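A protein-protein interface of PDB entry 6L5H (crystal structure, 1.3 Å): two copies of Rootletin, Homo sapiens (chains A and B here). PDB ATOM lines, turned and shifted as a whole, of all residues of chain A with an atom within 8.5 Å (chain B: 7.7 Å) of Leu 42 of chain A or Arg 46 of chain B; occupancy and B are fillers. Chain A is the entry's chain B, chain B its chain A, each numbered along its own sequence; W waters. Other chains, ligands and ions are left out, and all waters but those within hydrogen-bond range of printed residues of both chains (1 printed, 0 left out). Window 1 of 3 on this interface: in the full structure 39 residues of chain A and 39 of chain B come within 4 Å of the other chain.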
ATOM      1  N   LEU A  35      16.638   3.192 -27.810  1.00  0.00           N
ATOM      2  CA  LEU A  35      17.207   1.845 -27.743  1.00  0.00           C
ATOM      3  C   LEU A  35      17.583   1.326 -29.127  1.00  0.00           C
ATOM      4  O   LEU A  35      18.603   0.628 -29.281  1.00  0.00           O
ATOM      5  CB  LEU A  35      16.212   0.906 -27.054  1.00  0.00           C
ATOM      6  CG  LEU A  35      16.095   1.160 -25.552  1.00  0.00           C
ATOM      7  CD1 LEU A  35      14.919   0.391 -24.956  1.00  0.00           C
ATOM      8  CD2 LEU A  35      17.398   0.786 -24.853  1.00  0.00           C
ATOM      9  N   GLN A  36      16.784   1.660 -30.145  1.00  0.00           N
ATOM     10  CA  GLN A  36      17.075   1.229 -31.511  1.00  0.00           C
ATOM     11  C   GLN A  36      18.359   1.864 -32.029  1.00  0.00           C
ATOM     12  O   GLN A  36      19.189   1.192 -32.664  1.00  0.00           O
ATOM     13  CB  GLN A  36      15.902   1.580 -32.428  1.00  0.00           C
ATOM     14  CG  GLN A  36      14.686   0.706 -32.228  1.00  0.00           C
ATOM     15  CD  GLN A  36      13.530   1.136 -33.099  1.00  0.00           C
ATOM     16  OE1 GLN A  36      13.308   2.327 -33.307  1.00  0.00           O
ATOM     17  NE2 GLN A  36      12.802   0.167 -33.638  1.00  0.00           N
ATOM     18  N   GLU A  37      18.548   3.154 -31.760  1.00  0.00           N
ATOM     19  CA  GLU A  37      19.778   3.787 -32.214  1.00  0.00           C
ATOM     20  C   GLU A  37      20.973   3.272 -31.423  1.00  0.00           C
ATOM     21  O   GLU A  37      22.066   3.097 -31.981  1.00  0.00           O
ATOM     22  CB  GLU A  37      19.655   5.309 -32.131  1.00  0.00           C
ATOM     23  CG  GLU A  37      18.779   5.886 -33.232  1.00  0.00           C
ATOM     24  CD  GLU A  37      19.113   5.320 -34.605  1.00  0.00           C
ATOM     25  OE1 GLU A  37      20.273   5.478 -35.064  1.00  0.00           O
ATOM     26  OE2 GLU A  37      18.218   4.697 -35.222  1.00  0.00           O
ATOM     27  N   GLN A  38      20.778   2.990 -30.131  1.00  0.00           N
ATOM     28  CA  GLN A  38      21.846   2.379 -29.347  1.00  0.00           C
ATOM     29  C   GLN A  38      22.301   1.060 -29.961  1.00  0.00           C
ATOM     30  O   GLN A  38      23.509   0.798 -30.073  1.00  0.00           O
ATOM     31  CB  GLN A  38      21.373   2.173 -27.911  1.00  0.00           C
ATOM     32  CG  GLN A  38      22.351   1.412 -27.074  1.00  0.00           C
ATOM     33  CD  GLN A  38      22.003   1.447 -25.608  1.00  0.00           C
ATOM     34  OE1 GLN A  38      20.926   1.019 -25.204  1.00  0.00           O
ATOM     35  NE2 GLN A  38      22.922   1.951 -24.797  1.00  0.00           N
ATOM     36  N   ALA A  39      21.350   0.221 -30.373  1.00  0.00           N
ATOM     37  CA  ALA A  39      21.705  -1.052 -30.991  1.00  0.00           C
ATOM     38  C   ALA A  39      22.447  -0.837 -32.304  1.00  0.00           C
ATOM     39  O   ALA A  39      23.473  -1.479 -32.563  1.00  0.00           O
ATOM     40  CB  ALA A  39      20.454  -1.899 -31.221  1.00  0.00           C
ATOM     41  N   ARG A  40      21.932   0.051 -33.160  1.00  0.00           N
ATOM     42  CA  ARG A  40      22.592   0.293 -34.442  1.00  0.00           C
ATOM     43  C   ARG A  40      24.032   0.758 -34.235  1.00  0.00           C
ATOM     44  O   ARG A  40      24.959   0.287 -34.915  1.00  0.00           O
ATOM     45  CB  ARG A  40      21.792   1.315 -35.252  1.00  0.00           C
ATOM     46  CG  ARG A  40      22.119   1.358 -36.735  1.00  0.00           C
ATOM     47  CD  ARG A  40      20.854   1.545 -37.571  1.00  0.00           C
ATOM     48  NE  ARG A  40      20.192   0.272 -37.856  1.00  0.00           N
ATOM     49  CZ  ARG A  40      19.073   0.148 -38.566  1.00  0.00           C
ATOM     50  NH1 ARG A  40      18.479   1.224 -39.065  1.00  0.00           N
ATOM     51  NH2 ARG A  40      18.546  -1.052 -38.778  1.00  0.00           N
ATOM     52  N   ASP A  41      24.250   1.633 -33.249  1.00  0.00           N
ATOM     53  CA  ASP A  41      25.590   2.169 -33.017  1.00  0.00           C
ATOM     54  C   ASP A  41      26.523   1.137 -32.390  1.00  0.00           C
ATOM     55  O   ASP A  41      27.709   1.078 -32.742  1.00  0.00           O
ATOM     56  CB  ASP A  41      25.503   3.419 -32.142  1.00  0.00           C
ATOM     57  CG  ASP A  41      26.808   3.735 -31.434  1.00  0.00           C
ATOM     58  OD1 ASP A  41      26.917   3.419 -30.230  1.00  0.00           O
ATOM     59  OD2 ASP A  41      27.733   4.280 -32.081  1.00  0.00           O
ATOM     60  N   LEU A  42      26.026   0.335 -31.442  1.00  0.00           N
ATOM     61  CA  LEU A  42      26.860  -0.734 -30.890  1.00  0.00           C
ATOM     62  C   LEU A  42      27.249  -1.727 -31.972  1.00  0.00           C
ATOM     63  O   LEU A  42      28.386  -2.224 -31.989  1.00  0.00           O
ATOM     64  CB  LEU A  42      26.134  -1.440 -29.744  1.00  0.00           C
ATOM     65  CG  LEU A  42      26.000  -0.614 -28.460  1.00  0.00           C
ATOM     66  CD1 LEU A  42      25.099  -1.311 -27.448  1.00  0.00           C
ATOM     67  CD2 LEU A  42      27.379  -0.340 -27.872  1.00  0.00           C
ATOM     68  N   GLY A  43      26.327  -2.020 -32.892  1.00  0.00           N
ATOM     69  CA  GLY A  43      26.648  -2.910 -33.993  1.00  0.00           C
ATOM     70  C   GLY A  43      27.698  -2.327 -34.913  1.00  0.00           C
ATOM     71  O   GLY A  43      28.582  -3.043 -35.398  1.00  0.00           O
ATOM     72  N   LYS A  44      27.636  -1.015 -35.148  1.00  0.00           N
ATOM     73  CA  LYS A  44      28.665  -0.383 -35.970  1.00  0.00           C
ATOM     74  C   LYS A  44      30.027  -0.404 -35.274  1.00  0.00           C
ATOM     75  O   LYS A  44      31.046  -0.716 -35.910  1.00  0.00           O
ATOM     76  CB  LYS A  44      28.241   1.042 -36.332  1.00  0.00           C
ATOM     77  CG  LYS A  44      27.071   1.078 -37.301  1.00  0.00           C
ATOM     78  CD  LYS A  44      26.800   2.479 -37.836  1.00  0.00           C
ATOM     79  CE  LYS A  44      25.575   2.484 -38.748  1.00  0.00           C
ATOM     80  NZ  LYS A  44      25.028   3.853 -38.992  1.00  0.00           N
ATOM     81  N   GLN A  45      30.068  -0.073 -33.974  1.00  0.00           N
ATOM     82  CA  GLN A  45      31.322  -0.170 -33.222  1.00  0.00           C
ATOM     83  C   GLN A  45      31.879  -1.580 -33.276  1.00  0.00           C
ATOM     84  O   GLN A  45      33.094  -1.772 -33.445  1.00  0.00           O
ATOM     85  CB  GLN A  45      31.111   0.242 -31.766  1.00  0.00           C
ATOM     86  CG  GLN A  45      30.784   1.701 -31.557  1.00  0.00           C
ATOM     87  CD  GLN A  45      30.642   2.052 -30.091  1.00  0.00           C
ATOM     88  OE1 GLN A  45      31.438   1.625 -29.257  1.00  0.00           O
ATOM     89  NE2 GLN A  45      29.618   2.829 -29.768  1.00  0.00           N
ATOM     90  N   ARG A  46      31.008  -2.577 -33.130  1.00  0.00           N
ATOM     91  CA  ARG A  46      31.442  -3.967 -33.184  1.00  0.00           C
ATOM     92  C   ARG A  46      32.062  -4.303 -34.530  1.00  0.00           C
ATOM     93  O   ARG A  46      33.161  -4.860 -34.591  1.00  0.00           O
ATOM     94  CB  ARG A  46      30.264  -4.896 -32.912  1.00  0.00           C
ATOM     95  CG  ARG A  46      30.623  -6.364 -33.113  1.00  0.00           C
ATOM     96  CD  ARG A  46      29.364  -7.164 -33.360  1.00  0.00           C
ATOM     97  NE  ARG A  46      28.730  -6.770 -34.612  1.00  0.00           N
ATOM     98  CZ  ARG A  46      27.457  -7.003 -34.931  1.00  0.00           C
ATOM     99  NH1 ARG A  46      26.644  -7.634 -34.092  1.00  0.00           N
ATOM    100  NH2 ARG A  46      27.000  -6.595 -36.096  1.00  0.00           N
ATOM    101  N   ASP A  47      31.359  -3.995 -35.624  1.00  0.00           N
ATOM    102  CA  ASP A  47      31.859  -4.360 -36.948  1.00  0.00           C
ATOM    103  C   ASP A  47      33.185  -3.653 -37.250  1.00  0.00           C
ATOM    104  O   ASP A  47      34.109  -4.245 -37.838  1.00  0.00           O
ATOM    105  CB  ASP A  47      30.786  -4.047 -38.001  1.00  0.00           C
ATOM    106  CG  ASP A  47      29.539  -4.908 -37.835  1.00  0.00           C
ATOM    107  OD1 ASP A  47      29.617  -5.946 -37.139  1.00  0.00           O
ATOM    108  OD2 ASP A  47      28.479  -4.556 -38.400  1.00  0.00           O
ATOM    109  N   SER A  48      33.310  -2.401 -36.806  1.00  0.00           N
ATOM    110  CA  SER A  48      34.541  -1.646 -36.994  1.00  0.00           C
ATOM    111  C   SER A  48      35.707  -2.298 -36.258  1.00  0.00           C
ATOM    112  O   SER A  48      36.804  -2.491 -36.820  1.00  0.00           O
ATOM    113  CB  SER A  48      34.325  -0.222 -36.500  1.00  0.00           C
ATOM    114  OG  SER A  48      35.533   0.486 -36.387  1.00  0.00           O
ATOM    115  N   CYS A  49      35.492  -2.637 -34.984  1.00  0.00           N
ATOM    116  CA  CYS A  49      36.527  -3.330 -34.229  1.00  0.00           C
ATOM    117  C   CYS A  49      36.878  -4.660 -34.883  1.00  0.00           C
ATOM    118  O   CYS A  49      38.047  -5.065 -34.890  1.00  0.00           O
ATOM    119  CB  CYS A  49      36.079  -3.531 -32.779  1.00  0.00           C
ATOM    120  SG  CYS A  49      37.191  -4.577 -31.812  1.00  0.00           S
ATOM    121  N   LEU A  50      35.888  -5.370 -35.417  1.00  0.00           N
ATOM    122  CA  LEU A  50      36.162  -6.639 -36.088  1.00  0.00           C
ATOM    123  C   LEU A  50      37.137  -6.451 -37.246  1.00  0.00           C
ATOM    124  O   LEU A  50      38.068  -7.255 -37.434  1.00  0.00           O
ATOM    125  CB  LEU A  50      34.858  -7.264 -36.579  1.00  0.00           C
ATOM    126  CG  LEU A  50      33.970  -7.773 -35.447  1.00  0.00           C
ATOM    127  CD1 LEU A  50      32.614  -8.177 -35.995  1.00  0.00           C
ATOM    128  CD2 LEU A  50      34.622  -8.926 -34.707  1.00  0.00           C
ATOM    129  N   GLN B  36      16.230  -3.585 -24.922  1.00  0.00           N
ATOM    130  CA  GLN B  36      17.336  -3.526 -23.967  1.00  0.00           C
ATOM    131  C   GLN B  36      18.207  -4.769 -24.070  1.00  0.00           C
ATOM    132  O   GLN B  36      19.444  -4.689 -24.004  1.00  0.00           O
ATOM    133  CB  GLN B  36      16.795  -3.378 -22.546  1.00  0.00           C
ATOM    134  CG  GLN B  36      16.183  -2.025 -22.248  1.00  0.00           C
ATOM    135  CD  GLN B  36      15.554  -1.966 -20.871  1.00  0.00           C
ATOM    136  OE1 GLN B  36      15.103  -2.979 -20.337  1.00  0.00           O
ATOM    137  NE2 GLN B  36      15.521  -0.774 -20.287  1.00  0.00           N
ATOM    138  N   GLN B  38      18.629  -6.606 -26.764  1.00  0.00           N
ATOM    139  CA  GLN B  38      19.396  -6.472 -28.001  1.00  0.00           C
ATOM    140  C   GLN B  38      20.611  -5.573 -27.802  1.00  0.00           C
ATOM    141  O   GLN B  38      21.720  -5.889 -28.273  1.00  0.00           O
ATOM    142  CB  GLN B  38      18.509  -5.920 -29.122  1.00  0.00           C
ATOM    143  CG  GLN B  38      19.265  -5.737 -30.440  1.00  0.00           C
ATOM    144  CD  GLN B  38      18.481  -4.959 -31.489  1.00  0.00           C
ATOM    145  OE1 GLN B  38      17.501  -4.274 -31.178  1.00  0.00           O
ATOM    146  NE2 GLN B  38      18.921  -5.053 -32.739  1.00  0.00           N
ATOM    147  N   ALA B  39      20.426  -4.451 -27.105  1.00  0.00           N
ATOM    148  CA  ALA B  39      21.546  -3.550 -26.851  1.00  0.00           C
ATOM    149  C   ALA B  39      22.604  -4.226 -25.990  1.00  0.00           C
ATOM    150  O   ALA B  39      23.806  -4.053 -26.224  1.00  0.00           O
ATOM    151  CB  ALA B  39      21.048  -2.262 -26.195  1.00  0.00           C
ATOM    152  N   ARG B  40      22.184  -5.015 -24.998  1.00  0.00           N
ATOM    153  CA  ARG B  40      23.160  -5.753 -24.192  1.00  0.00           C
ATOM    154  C   ARG B  40      23.931  -6.765 -25.035  1.00  0.00           C
ATOM    155  O   ARG B  40      25.164  -6.873 -24.917  1.00  0.00           O
ATOM    156  CB  ARG B  40      22.457  -6.449 -23.023  1.00  0.00           C
ATOM    157  CG  ARG B  40      21.781  -5.488 -22.054  1.00  0.00           C
ATOM    158  CD  ARG B  40      21.117  -6.211 -20.886  1.00  0.00           C
ATOM    159  NE  ARG B  40      20.391  -5.279 -20.024  1.00  0.00           N
ATOM    160  CZ  ARG B  40      19.068  -5.262 -19.877  1.00  0.00           C
ATOM    161  NH1 ARG B  40      18.315  -6.141 -20.523  1.00  0.00           N
ATOM    162  NH2 ARG B  40      18.497  -4.372 -19.073  1.00  0.00           N
ATOM    163  N   ASP B  41      23.227  -7.513 -25.893  1.00  0.00           N
ATOM    164  CA  ASP B  41      23.870  -8.493 -26.779  1.00  0.00           C
ATOM    165  C   ASP B  41      24.934  -7.813 -27.631  1.00  0.00           C
ATOM    166  O   ASP B  41      26.106  -8.230 -27.654  1.00  0.00           O
ATOM    167  CB  ASP B  41      22.780  -9.182 -27.640  1.00  0.00           C
ATOM    168  CG  ASP B  41      23.322 -10.005 -28.858  1.00  0.00           C
ATOM    169  OD1 ASP B  41      24.545 -10.134 -29.074  1.00  0.00           O
ATOM    170  OD2 ASP B  41      22.476 -10.540 -29.632  1.00  0.00           O
ATOM    171  N   LEU B  42      24.548  -6.746 -28.316  1.00  0.00           N
ATOM    172  CA  LEU B  42      25.474  -6.046 -29.193  1.00  0.00           C
ATOM    173  C   LEU B  42      26.621  -5.427 -28.412  1.00  0.00           C
ATOM    174  O   LEU B  42      27.760  -5.396 -28.895  1.00  0.00           O
ATOM    175  CB  LEU B  42      24.708  -4.985 -29.977  1.00  0.00           C
ATOM    176  CG  LEU B  42      23.736  -5.672 -30.914  1.00  0.00           C
ATOM    177  CD1 LEU B  42      22.671  -4.683 -31.322  1.00  0.00           C
ATOM    178  CD2 LEU B  42      24.469  -6.210 -32.116  1.00  0.00           C
ATOM    179  N   GLY B  43      26.359  -4.947 -27.196  1.00  0.00           N
ATOM    180  CA  GLY B  43      27.433  -4.372 -26.402  1.00  0.00           C
ATOM    181  C   GLY B  43      28.449  -5.411 -25.974  1.00  0.00           C
ATOM    182  O   GLY B  43      29.649  -5.137 -25.952  1.00  0.00           O
ATOM    183  N   LYS B  44      27.983  -6.611 -25.619  1.00  0.00           N
ATOM    184  CA  LYS B  44      28.904  -7.689 -25.277  1.00  0.00           C
ATOM    185  C   LYS B  44      29.719  -8.102 -26.491  1.00  0.00           C
ATOM    186  O   LYS B  44      30.914  -8.413 -26.368  1.00  0.00           O
ATOM    187  CB  LYS B  44      28.137  -8.886 -24.712  1.00  0.00           C
ATOM    188  CG  LYS B  44      27.466  -8.638 -23.372  1.00  0.00           C
ATOM    189  CD  LYS B  44      28.343  -9.066 -22.206  1.00  0.00           C
ATOM    190  CE  LYS B  44      27.486  -9.650 -21.077  1.00  0.00           C
ATOM    191  NZ  LYS B  44      26.414  -8.721 -20.622  1.00  0.00           N
ATOM    192  N   GLN B  45      29.096  -8.120 -27.671  1.00  0.00           N
ATOM    193  CA  GLN B  45      29.845  -8.417 -28.893  1.00  0.00           C
ATOM    194  C   GLN B  45      30.933  -7.374 -29.116  1.00  0.00           C
ATOM    195  O   GLN B  45      32.100  -7.700 -29.398  1.00  0.00           O
ATOM    196  CB  GLN B  45      28.899  -8.475 -30.095  1.00  0.00           C
ATOM    197  CG  GLN B  45      27.909  -9.636 -30.081  1.00  0.00           C
ATOM    198  CD  GLN B  45      26.927  -9.564 -31.239  1.00  0.00           C
ATOM    199  OE1 GLN B  45      27.261  -9.087 -32.323  1.00  0.00           O
ATOM    200  NE2 GLN B  45      25.715 -10.039 -31.016  1.00  0.00           N
ATOM    201  N   ARG B  46      30.579  -6.114 -28.948  1.00  0.00           N
ATOM    202  CA  ARG B  46      31.550  -5.013 -29.103  1.00  0.00           C
ATOM    203  C   ARG B  46      32.668  -5.198 -28.070  1.00  0.00           C
ATOM    204  O   ARG B  46      33.822  -5.119 -28.469  1.00  0.00           O
ATOM    205  CB  ARG B  46      30.807  -3.697 -28.887  1.00  0.00           C
ATOM    206  CG  ARG B  46      31.654  -2.473 -29.173  1.00  0.00           C
ATOM    207  CD  ARG B  46      32.053  -1.654 -27.984  1.00  0.00           C
ATOM    208  NE  ARG B  46      31.506  -1.882 -26.669  1.00  0.00           N
ATOM    209  CZ  ARG B  46      30.874  -0.957 -25.989  1.00  0.00           C
ATOM    210  NH1 ARG B  46      30.673   0.215 -26.546  1.00  0.00           N
ATOM    211  NH2 ARG B  46      30.435  -1.206 -24.776  1.00  0.00           N
ATOM    212  N   ASP B  47      32.329  -5.456 -26.811  1.00  0.00           N
ATOM    213  CA  ASP B  47      33.337  -5.590 -25.761  1.00  0.00           C
ATOM    214  C   ASP B  47      34.282  -6.736 -26.056  1.00  0.00           C
ATOM    215  O   ASP B  47      35.494  -6.622 -25.833  1.00  0.00           O
ATOM    216  CB  ASP B  47      32.676  -5.821 -24.403  1.00  0.00           C
ATOM    217  CG  ASP B  47      31.979  -4.591 -23.878  1.00  0.00           C
ATOM    218  OD1 ASP B  47      32.175  -3.510 -24.468  1.00  0.00           O
ATOM    219  OD2 ASP B  47      31.227  -4.704 -22.879  1.00  0.00           O
ATOM    220  N   SER B  48      33.749  -7.861 -26.529  1.00  0.00           N
ATOM    221  CA  SER B  48      34.605  -9.009 -26.789  1.00  0.00           C
ATOM    222  C   SER B  48      35.605  -8.697 -27.890  1.00  0.00           C
ATOM    223  O   SER B  48      36.778  -9.088 -27.804  1.00  0.00           O
ATOM    224  CB  SER B  48      33.754 -10.225 -27.137  1.00  0.00           C
ATOM    225  OG  SER B  48      32.957 -10.572 -26.020  1.00  0.00           O
ATOM    226  N   CYS B  49      35.175  -7.955 -28.913  1.00  0.00           N
ATOM    227  CA  CYS B  49      36.133  -7.554 -29.935  1.00  0.00           C
ATOM    228  C   CYS B  49      37.183  -6.594 -29.372  1.00  0.00           C
ATOM    229  O   CYS B  49      38.371  -6.682 -29.726  1.00  0.00           O
ATOM    230  CB  CYS B  49      35.424  -6.924 -31.124  1.00  0.00           C
ATOM    231  SG  CYS B  49      36.639  -6.485 -32.369  1.00  0.00           S
ATOM    232  N   LEU B  50      36.762  -5.651 -28.523  1.00  0.00           N
ATOM    233  CA  LEU B  50      37.718  -4.726 -27.914  1.00  0.00           C
ATOM    234  C   LEU B  50      38.775  -5.484 -27.120  1.00  0.00           C
ATOM    235  O   LEU B  50      39.968  -5.149 -27.185  1.00  0.00           O
ATOM    236  CB  LEU B  50      37.003  -3.723 -27.009  1.00  0.00           C
ATOM    237  CG  LEU B  50      36.123  -2.696 -27.710  1.00  0.00           C
ATOM    238  CD1 LEU B  50      35.338  -1.902 -26.685  1.00  0.00           C
ATOM    239  CD2 LEU B  50      36.954  -1.759 -28.572  1.00  0.00           C
ATOM    240  N   ARG B  51      38.356  -6.521 -26.388  1.00  0.00           N
ATOM    241  CA  ARG B  51      39.295  -7.345 -25.629  1.00  0.00           C
ATOM    242  C   ARG B  51      40.273  -8.060 -26.558  1.00  0.00           C
ATOM    243  O   ARG B  51      41.491  -8.120 -26.285  1.00  0.00           O
ATOM    244  CB  ARG B  51      38.545  -8.376 -24.784  1.00  0.00           C
ATOM    245  CG  ARG B  51      37.572  -7.818 -23.758  1.00  0.00           C
ATOM    246  CD  ARG B  51      38.249  -7.009 -22.665  1.00  0.00           C
ATOM    247  NE  ARG B  51      38.492  -5.625 -23.051  1.00  0.00           N
ATOM    248  CZ  ARG B  51      37.577  -4.661 -22.975  1.00  0.00           C
ATOM    249  NH1 ARG B  51      37.889  -3.424 -23.344  1.00  0.00           N
ATOM    250  NH2 ARG B  51      36.345  -4.936 -22.543  1.00  0.00           N
ATOM    251  N   GLU B  52      39.750  -8.649 -27.647  1.00  0.00           N
ATOM    252  CA  GLU B  52      40.633  -9.325 -28.601  1.00  0.00           C
ATOM    253  C   GLU B  52      41.646  -8.350 -29.188  1.00  0.00           C
ATOM    254  O   GLU B  52      42.836  -8.670 -29.270  1.00  0.00           O
ATOM    255  CB  GLU B  52      39.844 -10.018 -29.730  1.00  0.00           C
ATOM    256  CG  GLU B  52      40.766 -10.900 -30.621  1.00  0.00           C
ATOM    257  CD  GLU B  52      40.074 -11.628 -31.781  1.00  0.00           C
ATOM    258  OE1 GLU B  52      38.829 -11.767 -31.783  1.00  0.00           O
ATOM    259  OE2 GLU B  52      40.801 -12.070 -32.705  1.00  0.00           O
HETATM  260  O   HOH W   1      17.980  -2.244 -29.031  1.00  0.00           O
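Leu 35 of chain A touches Gln 36 of chain B. CB of Ala 39 of chain B touches OE1 of Gln 38 of chain A, 3.4 Å away. CB of Ala 39 of chain A touches CD of Gln 38 of chain B, 3.7 Å away. O of Ala 39 of chain A touches CD1 of Leu 42 of chain B, 3.5 Å away. Ala 39 of chain B touches Leu 42 of chain A. CB of Leu 42 of chain B touches CB of Leu 42 of chain A (3.8 Å). Leu 42 of chain A touches Gly 43 of chain B. Arg 46 of chain B touches Leu 42 of chain A. Arg 46 of chain A touches Leu 42 of chain B.
Water W1 lies within hydrogen-bond range of O of Leu 35 of chain A (2.9 Å) and OE1 of Gln 38 of chain B (3.0 Å).
Of chain B, only Ala 39, Leu 42, Gly 43 and Arg 46 come within 4 Å of Leu 42 of chain A. Printed residues of chain A within 4 Å of Arg 46 of chain B: Leu 42 (3.6 Å) and Gln 45 (3.2 Å). No residue of chain B comes within 4 Å of Gly 43 of chain A. Gly 43 of chain B touches one residue of chain A. No residue of chain A comes within 4 Å of Asp 47 of chain B. Of the printed residues of chain A, Gln 38 of chain B touches Ala 39 (3.7 Å). Of the printed residues of chain B, Ala 39 of chain A touches Gln 38 and Leu 42. Of the printed residues of chain A, Leu 42 of chain B touches Ala 39 (3.5 Å), Leu 42 (3.8 Å) and Arg 46 (3.3 Å). Of the printed residues of chain B, Gln 45 of chain A touches Arg 46. Gln 36 of chain A touches none of the printed residues of chain B. Lys 44 of chain B touches none of the printed residues of chain A. The nearest residue of chain B that does not touch Leu 42 of chain A is Arg 40 of chain B (5.3 Å). The nearest printed residue of chain A that does not touch Arg 46 of chain B is Arg 46 of chain A (4.01 Å). The nearest printed residue of chain A that does not touch Gln 36 of chain B is Gln 38 of chain A (5.9 Å).
The guanidinium group of Arg 46 of chain B lies within salt-bridge range of the side-chain carboxylate of Asp 47 of chain B, at 2.8 Å. The side-chain carboxylate of Asp 47 of chain A lies within salt-bridge range of the guanidinium group of Arg 46 of chain A. NE2 of Gln 45 of chain A is in hydrogen-bond range of OD1 of Asp 41 of chain A.
Hydrophobic or aromatic side chains of chain A that line the printed part of chain B: Leu 35, Ala 39, Leu 42 and Leu 50. Along chain A the printed residues that touch a printed residue of chain B span positions 35 to 50. Printed residues of chain B that touch a printed residue of chain A: Gln 36, Gln 38, Ala 39, Leu 42, Gly 43, Gln 45, Arg 46, Cys 49 and Leu 50. Hydrophobic or aromatic side chains of chain B that line the printed part of chain A: Ala 39 and Leu 42. Among the printed residues, no Asp or Glu carboxylate lies within 4 Å of a Lys or Arg side-chain nitrogen of the other chain.
SG of Cys 49 of chain A sits at hydrogen-bond distance from N of Leu 50 of chain B, 3.5 Å away. The side-chain sulfur of Cys 49 of chain B is in hydrogen-bond range of the backbone NH of Leu 50 of chain A. The side-chain amide oxygen (OE1) of Gln 45 of chain A sits at hydrogen-bond distance from the guanidinium group (NH1) of Arg 46 of chain B, at 3.2 Å. OE1 of Gln 45 of chain B lies close to NH1 of Arg 46 of chain A. The side-chain sulfur (SG) of Cys 49 of chain B forms a disulfide with the side-chain sulfur (SG) of Cys 49 of chain A.
Ala 39 of chain A touches Leu 42 of chain B, and with the chains exchanged Leu 42 of chain A touches Ala 39 of chain B. Leu 42 of chain B touches its own counterpart, Leu 42 of chain A. Leu 42 of chain A touches Gly 43 of chain B, but with the chains exchanged Gly 43 of chain A does not touch Leu 42 of chain B (4.4 Å). Leu 42 of chain A touches Arg 46 of chain B, and with the chains exchanged Arg 46 of chain A touches Leu 42 of chain B.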
